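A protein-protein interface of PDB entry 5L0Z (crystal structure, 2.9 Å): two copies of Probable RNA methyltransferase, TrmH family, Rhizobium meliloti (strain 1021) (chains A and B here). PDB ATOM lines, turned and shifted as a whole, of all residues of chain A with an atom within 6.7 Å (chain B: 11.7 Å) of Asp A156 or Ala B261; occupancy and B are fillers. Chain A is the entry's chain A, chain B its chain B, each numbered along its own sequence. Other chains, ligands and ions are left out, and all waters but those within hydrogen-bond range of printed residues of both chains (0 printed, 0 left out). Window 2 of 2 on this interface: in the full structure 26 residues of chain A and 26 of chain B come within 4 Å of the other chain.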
ATOM      1  N   ILE A 151       8.256 -21.448 -33.183  1.00  0.00           N
ATOM      2  CA  ILE A 151       9.448 -20.902 -33.795  1.00  0.00           C
ATOM      3  C   ILE A 151       9.479 -19.364 -33.719  1.00  0.00           C
ATOM      4  O   ILE A 151      10.535 -18.750 -33.528  1.00  0.00           O
ATOM      5  CB  ILE A 151       9.554 -21.414 -35.223  1.00  0.00           C
ATOM      6  CG1 ILE A 151       9.979 -22.884 -35.164  1.00  0.00           C
ATOM      7  CG2 ILE A 151      10.596 -20.639 -35.999  1.00  0.00           C
ATOM      8  CD1 ILE A 151       9.750 -23.687 -36.420  1.00  0.00           C
ATOM      9  N   ILE A 152       8.300 -18.755 -33.825  1.00  0.00           N
ATOM     10  CA  ILE A 152       8.191 -17.324 -33.914  1.00  0.00           C
ATOM     11  C   ILE A 152       8.446 -16.751 -32.567  1.00  0.00           C
ATOM     12  O   ILE A 152       9.173 -15.829 -32.432  1.00  0.00           O
ATOM     13  CB  ILE A 152       6.822 -16.890 -34.475  1.00  0.00           C
ATOM     14  CG1 ILE A 152       6.792 -17.144 -35.985  1.00  0.00           C
ATOM     15  CG2 ILE A 152       6.548 -15.392 -34.197  1.00  0.00           C
ATOM     16  CD1 ILE A 152       5.384 -17.229 -36.516  1.00  0.00           C
ATOM     17  N   ARG A 153       7.809 -17.313 -31.588  1.00  0.00           N
ATOM     18  CA  ARG A 153       8.120 -17.065 -30.204  1.00  0.00           C
ATOM     19  C   ARG A 153       9.593 -17.233 -29.796  1.00  0.00           C
ATOM     20  O   ARG A 153      10.105 -16.530 -28.920  1.00  0.00           O
ATOM     21  CB  ARG A 153       7.287 -18.046 -29.399  1.00  0.00           C
ATOM     22  CG  ARG A 153       7.359 -17.845 -27.923  1.00  0.00           C
ATOM     23  CD  ARG A 153       6.317 -18.702 -27.254  1.00  0.00           C
ATOM     24  NE  ARG A 153       6.562 -18.697 -25.821  1.00  0.00           N
ATOM     25  CZ  ARG A 153       6.283 -19.697 -24.994  1.00  0.00           C
ATOM     26  NH1 ARG A 153       5.706 -20.819 -25.423  1.00  0.00           N
ATOM     27  NH2 ARG A 153       6.592 -19.567 -23.709  1.00  0.00           N
ATOM     28  N   THR A 154      10.250 -18.211 -30.389  1.00  0.00           N
ATOM     29  CA  THR A 154      11.579 -18.625 -29.950  1.00  0.00           C
ATOM     30  C   THR A 154      12.656 -17.791 -30.630  1.00  0.00           C
ATOM     31  O   THR A 154      13.689 -17.473 -30.013  1.00  0.00           O
ATOM     32  CB  THR A 154      11.795 -20.121 -30.251  1.00  0.00           C
ATOM     33  OG1 THR A 154      10.749 -20.858 -29.650  1.00  0.00           O
ATOM     34  CG2 THR A 154      13.107 -20.637 -29.669  1.00  0.00           C
ATOM     35  N   ALA A 155      12.430 -17.509 -31.913  1.00  0.00           N
ATOM     36  CA  ALA A 155      13.225 -16.572 -32.661  1.00  0.00           C
ATOM     37  C   ALA A 155      13.220 -15.193 -31.999  1.00  0.00           C
ATOM     38  O   ALA A 155      14.263 -14.548 -31.915  1.00  0.00           O
ATOM     39  CB  ALA A 155      12.692 -16.479 -34.074  1.00  0.00           C
ATOM     40  N   ASP A 156      12.050 -14.767 -31.517  1.00  0.00           N
ATOM     41  CA  ASP A 156      11.878 -13.496 -30.787  1.00  0.00           C
ATOM     42  C   ASP A 156      12.739 -13.547 -29.545  1.00  0.00           C
ATOM     43  O   ASP A 156      13.593 -12.664 -29.310  1.00  0.00           O
ATOM     44  CB  ASP A 156      10.397 -13.315 -30.408  1.00  0.00           C
ATOM     45  CG  ASP A 156      10.087 -11.986 -29.667  1.00  0.00           C
ATOM     46  OD1 ASP A 156      10.536 -10.869 -30.089  1.00  0.00           O
ATOM     47  OD2 ASP A 156       9.323 -12.060 -28.665  1.00  0.00           O
ATOM     48  N   ALA A 157      12.546 -14.625 -28.779  1.00  0.00           N
ATOM     49  CA  ALA A 157      13.319 -14.860 -27.555  1.00  0.00           C
ATOM     50  C   ALA A 157      14.863 -14.882 -27.760  1.00  0.00           C
ATOM     51  O   ALA A 157      15.607 -14.474 -26.874  1.00  0.00           O
ATOM     52  CB  ALA A 157      12.840 -16.128 -26.894  1.00  0.00           C
ATOM     53  N   ALA A 158      15.332 -15.331 -28.923  1.00  0.00           N
ATOM     54  CA  ALA A 158      16.766 -15.425 -29.184  1.00  0.00           C
ATOM     55  C   ALA A 158      17.358 -14.093 -29.684  1.00  0.00           C
ATOM     56  O   ALA A 158      18.569 -14.005 -29.944  1.00  0.00           O
ATOM     57  CB  ALA A 158      17.031 -16.522 -30.196  1.00  0.00           C
ATOM     58  N   GLY A 159      16.511 -13.068 -29.841  1.00  0.00           N
ATOM     59  CA  GLY A 159      16.899 -11.854 -30.541  1.00  0.00           C
ATOM     60  C   GLY A 159      17.238 -12.015 -32.009  1.00  0.00           C
ATOM     61  O   GLY A 159      18.146 -11.349 -32.497  1.00  0.00           O
ATOM     62  N   ALA A 160      16.516 -12.876 -32.723  1.00  0.00           N
ATOM     63  CA  ALA A 160      16.649 -12.947 -34.169  1.00  0.00           C
ATOM     64  C   ALA A 160      15.816 -11.810 -34.775  1.00  0.00           C
ATOM     65  O   ALA A 160      14.985 -11.205 -34.116  1.00  0.00           O
ATOM     66  CB  ALA A 160      16.218 -14.293 -34.704  1.00  0.00           C
ATOM     67  N   ILE A 163      11.628 -13.887 -39.582  1.00  0.00           N
ATOM     68  CA  ILE A 163      11.180 -15.199 -40.088  1.00  0.00           C
ATOM     69  C   ILE A 163      10.840 -15.035 -41.566  1.00  0.00           C
ATOM     70  O   ILE A 163      10.070 -14.161 -41.935  1.00  0.00           O
ATOM     71  CB  ILE A 163       9.895 -15.676 -39.366  1.00  0.00           C
ATOM     72  CG1 ILE A 163      10.057 -15.615 -37.844  1.00  0.00           C
ATOM     73  CG2 ILE A 163       9.471 -17.062 -39.823  1.00  0.00           C
ATOM     74  CD1 ILE A 163      11.180 -16.454 -37.279  1.00  0.00           C
ATOM     75  N   THR A 181       2.442 -18.348 -30.603  1.00  0.00           N
ATOM     76  CA  THR A 181       3.503 -17.371 -30.525  1.00  0.00           C
ATOM     77  C   THR A 181       3.595 -16.729 -29.177  1.00  0.00           C
ATOM     78  O   THR A 181       4.625 -16.148 -28.853  1.00  0.00           O
ATOM     79  CB  THR A 181       3.346 -16.209 -31.531  1.00  0.00           C
ATOM     80  OG1 THR A 181       2.127 -15.526 -31.287  1.00  0.00           O
ATOM     81  CG2 THR A 181       3.355 -16.694 -32.931  1.00  0.00           C
ATOM     82  N   MET A 182       2.507 -16.774 -28.420  1.00  0.00           N
ATOM     83  CA  MET A 182       2.392 -16.039 -27.143  1.00  0.00           C
ATOM     84  C   MET A 182       2.749 -14.569 -27.254  1.00  0.00           C
ATOM     85  O   MET A 182       3.479 -14.045 -26.406  1.00  0.00           O
ATOM     86  CB  MET A 182       3.258 -16.664 -26.066  1.00  0.00           C
ATOM     87  CG  MET A 182       3.022 -18.162 -25.986  1.00  0.00           C
ATOM     88  SD  MET A 182       1.682 -18.478 -24.620  1.00  0.00           S
ATOM     89  CE  MET A 182       2.782 -17.918 -23.051  1.00  0.00           C
ATOM     90  N   GLY A 183       2.236 -13.893 -28.285  1.00  0.00           N
ATOM     91  CA  GLY A 183       2.475 -12.484 -28.488  1.00  0.00           C
ATOM     92  C   GLY A 183       3.574 -12.148 -29.497  1.00  0.00           C
ATOM     93  O   GLY A 183       3.611 -11.022 -30.048  1.00  0.00           O
ATOM     94  N   SER A 184       4.458 -13.097 -29.791  1.00  0.00           N
ATOM     95  CA  SER A 184       5.602 -12.783 -30.626  1.00  0.00           C
ATOM     96  C   SER A 184       5.278 -12.553 -32.110  1.00  0.00           C
ATOM     97  O   SER A 184       6.137 -12.168 -32.874  1.00  0.00           O
ATOM     98  CB  SER A 184       6.674 -13.853 -30.451  1.00  0.00           C
ATOM     99  OG  SER A 184       7.163 -13.852 -29.113  1.00  0.00           O
ATOM    100  N   VAL A 185       4.050 -12.765 -32.538  1.00  0.00           N
ATOM    101  CA  VAL A 185       3.687 -12.467 -33.922  1.00  0.00           C
ATOM    102  C   VAL A 185       3.760 -10.961 -34.207  1.00  0.00           C
ATOM    103  O   VAL A 185       4.112 -10.514 -35.320  1.00  0.00           O
ATOM    104  CB  VAL A 185       2.304 -13.030 -34.260  1.00  0.00           C
ATOM    105  CG1 VAL A 185       1.213 -12.350 -33.435  1.00  0.00           C
ATOM    106  CG2 VAL A 185       2.042 -12.909 -35.753  1.00  0.00           C
ATOM    107  N   ALA A 187       5.919  -9.038 -32.628  1.00  0.00           N
ATOM    108  CA  ALA A 187       7.223  -8.534 -32.215  1.00  0.00           C
ATOM    109  C   ALA A 187       8.346  -8.903 -33.131  1.00  0.00           C
ATOM    110  O   ALA A 187       9.413  -8.379 -32.925  1.00  0.00           O
ATOM    111  CB  ALA A 187       7.557  -8.990 -30.803  1.00  0.00           C
ATOM    112  N   ILE A 188       8.156  -9.778 -34.122  1.00  0.00           N
ATOM    113  CA  ILE A 188       9.253 -10.091 -35.057  1.00  0.00           C
ATOM    114  C   ILE A 188       8.779 -10.146 -36.531  1.00  0.00           C
ATOM    115  O   ILE A 188       7.766 -10.791 -36.834  1.00  0.00           O
ATOM    116  CB  ILE A 188       9.990 -11.377 -34.616  1.00  0.00           C
ATOM    117  CG1 ILE A 188      10.951 -11.860 -35.712  1.00  0.00           C
ATOM    118  CG2 ILE A 188       8.985 -12.457 -34.232  1.00  0.00           C
ATOM    119  CD1 ILE A 188      11.945 -12.928 -35.294  1.00  0.00           C
ATOM    120  N   LEU A 274      18.959 -21.759 -33.061  1.00  0.00           N
ATOM    121  CA  LEU A 274      18.943 -20.356 -32.703  1.00  0.00           C
ATOM    122  C   LEU A 274      19.972 -20.038 -31.644  1.00  0.00           C
ATOM    123  O   LEU A 274      20.672 -19.057 -31.737  1.00  0.00           O
ATOM    124  CB  LEU A 274      17.592 -19.930 -32.217  1.00  0.00           C
ATOM    125  CG  LEU A 274      16.714 -19.548 -33.391  1.00  0.00           C
ATOM    126  CD1 LEU A 274      15.242 -19.607 -32.954  1.00  0.00           C
ATOM    127  CD2 LEU A 274      17.086 -18.166 -33.970  1.00  0.00           C
ATOM    128  N   HIS B 213      15.299 -22.418 -13.676  1.00  0.00           N
ATOM    129  CA  HIS B 213      14.622 -21.456 -12.818  1.00  0.00           C
ATOM    130  C   HIS B 213      14.868 -20.139 -13.473  1.00  0.00           C
ATOM    131  O   HIS B 213      15.397 -20.105 -14.586  1.00  0.00           O
ATOM    132  CB  HIS B 213      15.267 -21.455 -11.417  1.00  0.00           C
ATOM    133  CG  HIS B 213      14.291 -21.315 -10.284  1.00  0.00           C
ATOM    134  ND1 HIS B 213      13.646 -20.135  -9.967  1.00  0.00           N
ATOM    135  CD2 HIS B 213      13.860 -22.230  -9.380  1.00  0.00           C
ATOM    136  CE1 HIS B 213      12.856 -20.335  -8.926  1.00  0.00           C
ATOM    137  NE2 HIS B 213      12.968 -21.597  -8.551  1.00  0.00           N
ATOM    138  N   LEU B 214      14.456 -19.058 -12.814  1.00  0.00           N
ATOM    139  CA  LEU B 214      15.086 -17.737 -13.005  1.00  0.00           C
ATOM    140  C   LEU B 214      15.696 -17.125 -11.670  1.00  0.00           C
ATOM    141  O   LEU B 214      16.142 -15.969 -11.697  1.00  0.00           O
ATOM    142  CB  LEU B 214      14.086 -16.788 -13.725  1.00  0.00           C
ATOM    143  CG  LEU B 214      13.513 -17.077 -15.158  1.00  0.00           C
ATOM    144  CD1 LEU B 214      14.632 -17.102 -16.179  1.00  0.00           C
ATOM    145  CD2 LEU B 214      12.628 -18.318 -15.363  1.00  0.00           C
ATOM    146  N   GLU B 237       4.556 -25.194 -16.793  1.00  0.00           N
ATOM    147  CA  GLU B 237       4.383 -24.204 -17.855  1.00  0.00           C
ATOM    148  C   GLU B 237       3.908 -22.869 -17.334  1.00  0.00           C
ATOM    149  O   GLU B 237       4.362 -21.852 -17.820  1.00  0.00           O
ATOM    150  CB  GLU B 237       3.419 -24.710 -18.936  1.00  0.00           C
ATOM    151  CG  GLU B 237       3.992 -25.787 -19.851  1.00  0.00           C
ATOM    152  CD  GLU B 237       3.527 -27.203 -19.527  1.00  0.00           C
ATOM    153  OE1 GLU B 237       3.319 -27.577 -18.336  1.00  0.00           O
ATOM    154  OE2 GLU B 237       3.351 -27.969 -20.493  1.00  0.00           O
ATOM    155  N   ARG B 254      19.739 -21.060 -15.979  1.00  0.00           N
ATOM    156  CA  ARG B 254      18.913 -20.191 -16.750  1.00  0.00           C
ATOM    157  C   ARG B 254      19.536 -20.019 -18.138  1.00  0.00           C
ATOM    158  O   ARG B 254      20.751 -19.921 -18.286  1.00  0.00           O
ATOM    159  CB  ARG B 254      18.798 -18.874 -16.006  1.00  0.00           C
ATOM    160  CG  ARG B 254      18.072 -17.769 -16.730  1.00  0.00           C
ATOM    161  CD  ARG B 254      17.962 -16.554 -15.822  1.00  0.00           C
ATOM    162  NE  ARG B 254      17.803 -15.332 -16.609  1.00  0.00           N
ATOM    163  CZ  ARG B 254      17.975 -14.093 -16.150  1.00  0.00           C
ATOM    164  NH1 ARG B 254      18.294 -13.859 -14.879  1.00  0.00           N
ATOM    165  NH2 ARG B 254      17.816 -13.062 -16.976  1.00  0.00           N
ATOM    166  N   ILE B 255      18.675 -20.016 -19.144  1.00  0.00           N
ATOM    167  CA  ILE B 255      19.053 -19.784 -20.514  1.00  0.00           C
ATOM    168  C   ILE B 255      18.807 -18.288 -20.790  1.00  0.00           C
ATOM    169  O   ILE B 255      17.675 -17.827 -20.690  1.00  0.00           O
ATOM    170  CB  ILE B 255      18.185 -20.646 -21.456  1.00  0.00           C
ATOM    171  CG1 ILE B 255      18.274 -22.116 -21.082  1.00  0.00           C
ATOM    172  CG2 ILE B 255      18.610 -20.483 -22.905  1.00  0.00           C
ATOM    173  CD1 ILE B 255      17.298 -22.981 -21.824  1.00  0.00           C
ATOM    174  N   PRO B 256      19.850 -17.528 -21.156  1.00  0.00           N
ATOM    175  CA  PRO B 256      19.629 -16.107 -21.398  1.00  0.00           C
ATOM    176  C   PRO B 256      18.775 -15.867 -22.623  1.00  0.00           C
ATOM    177  O   PRO B 256      18.845 -16.642 -23.565  1.00  0.00           O
ATOM    178  CB  PRO B 256      21.044 -15.547 -21.650  1.00  0.00           C
ATOM    179  CG  PRO B 256      21.984 -16.698 -21.620  1.00  0.00           C
ATOM    180  CD  PRO B 256      21.159 -17.957 -21.674  1.00  0.00           C
ATOM    181  N   GLN B 257      17.990 -14.789 -22.599  1.00  0.00           N
ATOM    182  CA  GLN B 257      17.097 -14.408 -23.711  1.00  0.00           C
ATOM    183  C   GLN B 257      17.195 -12.908 -24.037  1.00  0.00           C
ATOM    184  O   GLN B 257      17.969 -12.190 -23.394  1.00  0.00           O
ATOM    185  CB  GLN B 257      15.653 -14.756 -23.378  1.00  0.00           C
ATOM    186  CG  GLN B 257      15.376 -16.177 -22.916  1.00  0.00           C
ATOM    187  CD  GLN B 257      13.905 -16.339 -22.596  1.00  0.00           C
ATOM    188  OE1 GLN B 257      13.046 -15.683 -23.182  1.00  0.00           O
ATOM    189  NE2 GLN B 257      13.610 -17.152 -21.644  1.00  0.00           N
ATOM    190  N   ALA B 258      16.425 -12.451 -25.029  1.00  0.00           N
ATOM    191  CA  ALA B 258      16.431 -11.064 -25.486  1.00  0.00           C
ATOM    192  C   ALA B 258      15.014 -10.609 -25.883  1.00  0.00           C
ATOM    193  O   ALA B 258      14.536 -10.936 -26.976  1.00  0.00           O
ATOM    194  CB  ALA B 258      17.375 -10.949 -26.665  1.00  0.00           C
ATOM    195  N   GLY B 259      14.324  -9.885 -24.998  1.00  0.00           N
ATOM    196  CA  GLY B 259      12.975  -9.336 -25.298  1.00  0.00           C
ATOM    197  C   GLY B 259      11.997  -9.239 -24.126  1.00  0.00           C
ATOM    198  O   GLY B 259      12.359  -9.487 -22.959  1.00  0.00           O
ATOM    199  N   ARG B 260      10.757  -8.845 -24.451  1.00  0.00           N
ATOM    200  CA  ARG B 260       9.626  -8.871 -23.501  1.00  0.00           C
ATOM    201  C   ARG B 260       9.205 -10.319 -23.304  1.00  0.00           C
ATOM    202  O   ARG B 260       8.644 -10.662 -22.257  1.00  0.00           O
ATOM    203  CB  ARG B 260       8.431  -8.021 -23.976  1.00  0.00           C
ATOM    204  N   ALA B 261       9.473 -11.161 -24.312  1.00  0.00           N
ATOM    205  CA  ALA B 261       9.316 -12.610 -24.192  1.00  0.00           C
ATOM    206  C   ALA B 261      10.049 -13.099 -22.950  1.00  0.00           C
ATOM    207  O   ALA B 261      11.284 -13.052 -22.905  1.00  0.00           O
ATOM    208  CB  ALA B 261       9.859 -13.299 -25.434  1.00  0.00           C
ATOM    209  N   ASP B 262       9.279 -13.535 -21.952  1.00  0.00           N
ATOM    210  CA  ASP B 262       9.793 -13.888 -20.600  1.00  0.00           C
ATOM    211  C   ASP B 262      10.219 -15.364 -20.434  1.00  0.00           C
ATOM    212  O   ASP B 262      11.124 -15.666 -19.641  1.00  0.00           O
ATOM    213  CB  ASP B 262       8.740 -13.560 -19.520  1.00  0.00           C
ATOM    214  CG  ASP B 262       7.401 -14.265 -19.770  1.00  0.00           C
ATOM    215  OD1 ASP B 262       7.221 -15.415 -19.313  1.00  0.00           O
ATOM    216  OD2 ASP B 262       6.547 -13.687 -20.475  1.00  0.00           O
ATOM    217  N   SER B 263       9.536 -16.268 -21.138  1.00  0.00           N
ATOM    218  CA  SER B 263       9.784 -17.693 -21.037  1.00  0.00           C
ATOM    219  C   SER B 263      10.074 -18.243 -22.409  1.00  0.00           C
ATOM    220  O   SER B 263       9.629 -17.691 -23.425  1.00  0.00           O
ATOM    221  CB  SER B 263       8.546 -18.408 -20.485  1.00  0.00           C
ATOM    222  OG  SER B 263       8.688 -18.705 -19.112  1.00  0.00           O
ATOM    223  N   LEU B 264      10.826 -19.338 -22.435  1.00  0.00           N
ATOM    224  CA  LEU B 264      10.806 -20.241 -23.574  1.00  0.00           C
ATOM    225  C   LEU B 264       9.694 -21.239 -23.281  1.00  0.00           C
ATOM    226  O   LEU B 264       9.422 -21.550 -22.128  1.00  0.00           O
ATOM    227  CB  LEU B 264      12.140 -20.970 -23.732  1.00  0.00           C
ATOM    228  CG  LEU B 264      13.371 -20.071 -23.938  1.00  0.00           C
ATOM    229  CD1 LEU B 264      14.680 -20.830 -23.809  1.00  0.00           C
ATOM    230  CD2 LEU B 264      13.297 -19.376 -25.280  1.00  0.00           C
ATOM    231  N   ASN B 265       9.009 -21.690 -24.325  1.00  0.00           N
ATOM    232  CA  ASN B 265       8.240 -22.913 -24.282  1.00  0.00           C
ATOM    233  C   ASN B 265       9.056 -23.951 -23.513  1.00  0.00           C
ATOM    234  O   ASN B 265      10.272 -24.035 -23.642  1.00  0.00           O
ATOM    235  CB  ASN B 265       7.986 -23.381 -25.714  1.00  0.00           C
ATOM    236  CG  ASN B 265       7.511 -24.797 -25.787  1.00  0.00           C
ATOM    237  OD1 ASN B 265       8.267 -25.695 -26.107  1.00  0.00           O
ATOM    238  ND2 ASN B 265       6.273 -25.011 -25.449  1.00  0.00           N
ATOM    239  N   ILE B 268      11.035 -26.453 -25.635  1.00  0.00           N
ATOM    240  CA  ILE B 268      12.153 -25.751 -26.253  1.00  0.00           C
ATOM    241  C   ILE B 268      13.225 -25.610 -25.190  1.00  0.00           C
ATOM    242  O   ILE B 268      14.341 -26.092 -25.380  1.00  0.00           O
ATOM    243  CB  ILE B 268      11.725 -24.380 -26.840  1.00  0.00           C
ATOM    244  CG1 ILE B 268      10.729 -24.582 -28.005  1.00  0.00           C
ATOM    245  CG2 ILE B 268      12.928 -23.555 -27.263  1.00  0.00           C
ATOM    246  CD1 ILE B 268      11.318 -24.908 -29.365  1.00  0.00           C
ATOM    247  N   ALA B 269      12.898 -24.998 -24.065  1.00  0.00           N
ATOM    248  CA  ALA B 269      13.871 -24.911 -22.989  1.00  0.00           C
ATOM    249  C   ALA B 269      14.516 -26.302 -22.753  1.00  0.00           C
ATOM    250  O   ALA B 269      15.752 -26.402 -22.818  1.00  0.00           O
ATOM    251  CB  ALA B 269      13.252 -24.363 -21.720  1.00  0.00           C
ATOM    252  N   ILE B 272      17.040 -27.413 -25.489  1.00  0.00           N
ATOM    253  CA  ILE B 272      18.297 -26.666 -25.262  1.00  0.00           C
ATOM    254  C   ILE B 272      19.128 -27.187 -24.084  1.00  0.00           C
ATOM    255  O   ILE B 272      20.335 -27.300 -24.191  1.00  0.00           O
ATOM    256  CB  ILE B 272      18.026 -25.165 -25.128  1.00  0.00           C
ATOM    257  CG1 ILE B 272      17.719 -24.630 -26.518  1.00  0.00           C
ATOM    258  CG2 ILE B 272      19.220 -24.408 -24.577  1.00  0.00           C
ATOM    259  CD1 ILE B 272      16.949 -23.323 -26.518  1.00  0.00           C
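Printed residues of chain B that touch a printed residue of chain A: Gln B257, Ala B258, Ala B261, Ser B263, Leu B264, Asn B265 and Ile B268. Hydrophobic or aromatic side chains of chain B within 4 Å of the printed part of chain A: Ala B258, Ala B261, Leu B264 and Ile B268. Of the 19 printed residues of chain A, 5 touch a printed residue of chain B. Among the printed residues, no Asp or Glu carboxylate lies within 4 Å of a Lys or Arg side-chain nitrogen of the other chain.
No position is printed for both chains. Of the 10 pairs that touch across the chains among the printed residues, none has its exchanged pair printed and touching as well.
Arg A153 touches Ser B263 (NH2 to O, 3.6 Å). Arg A153 touches Leu B264 (NH2 to C, 3.5 Å). Ile B268 touches Thr A154. Asp A156 touches Ala B261 (OD2 to CB, 3.5 Å). Ala A157 touches Gln B257 (O to CA, 3.5 Å). Leu B264 touches Ala A157 (CD2 to CB, 3.7 Å). CB of Ala B258 touches N of Gly A159, 3.9 Å away.
OG of Ser A184 lies within hydrogen-bond range of OD2 of Asp A156 (2.8 Å). The side-chain amide oxygen of Asn B265 is in hydrogen-bond range of the backbone NH of Ile B268 (2.9 Å). The side-chain amide oxygen of Gln B257 sits close to the backbone carbonyl oxygen of Ala B261, 3.2 Å away.
The backbone carbonyl oxygen (O) of Ala B258 sits close to the backbone carbonyl oxygen (O) of Asp A156 (3.1 Å). O of Ala A157 sits at hydrogen-bond distance from N of Ala B258 (2.9 Å). N of Asn B265 sits close to NH2 of Arg A153, 3.3 Å away.
Asp A156 touches just these residues of chain B: Ala B258 (3.1 Å) and Ala B261 (3.5 Å). Ala B261 touches one residue of chain A. Ala A155 touches none of the printed residues of chain B. Ala A157 touches just these residues of chain B: Gln B257, Ala B258 and Leu B264. No residue of chain B comes within 4 Å of Ala A158. Ala A187 touches none of the printed residues of chain B. Of the printed residues of chain A, Gln B257 touches Ala A157 (3.5 Å). Of the printed residues of chain A, Leu B264 touches Arg A153 (3.5 Å) and Ala A157 (3.7 Å). The nearest printed residue of chain B that does not touch Arg A153 is Ala B261 (4.8 Å).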
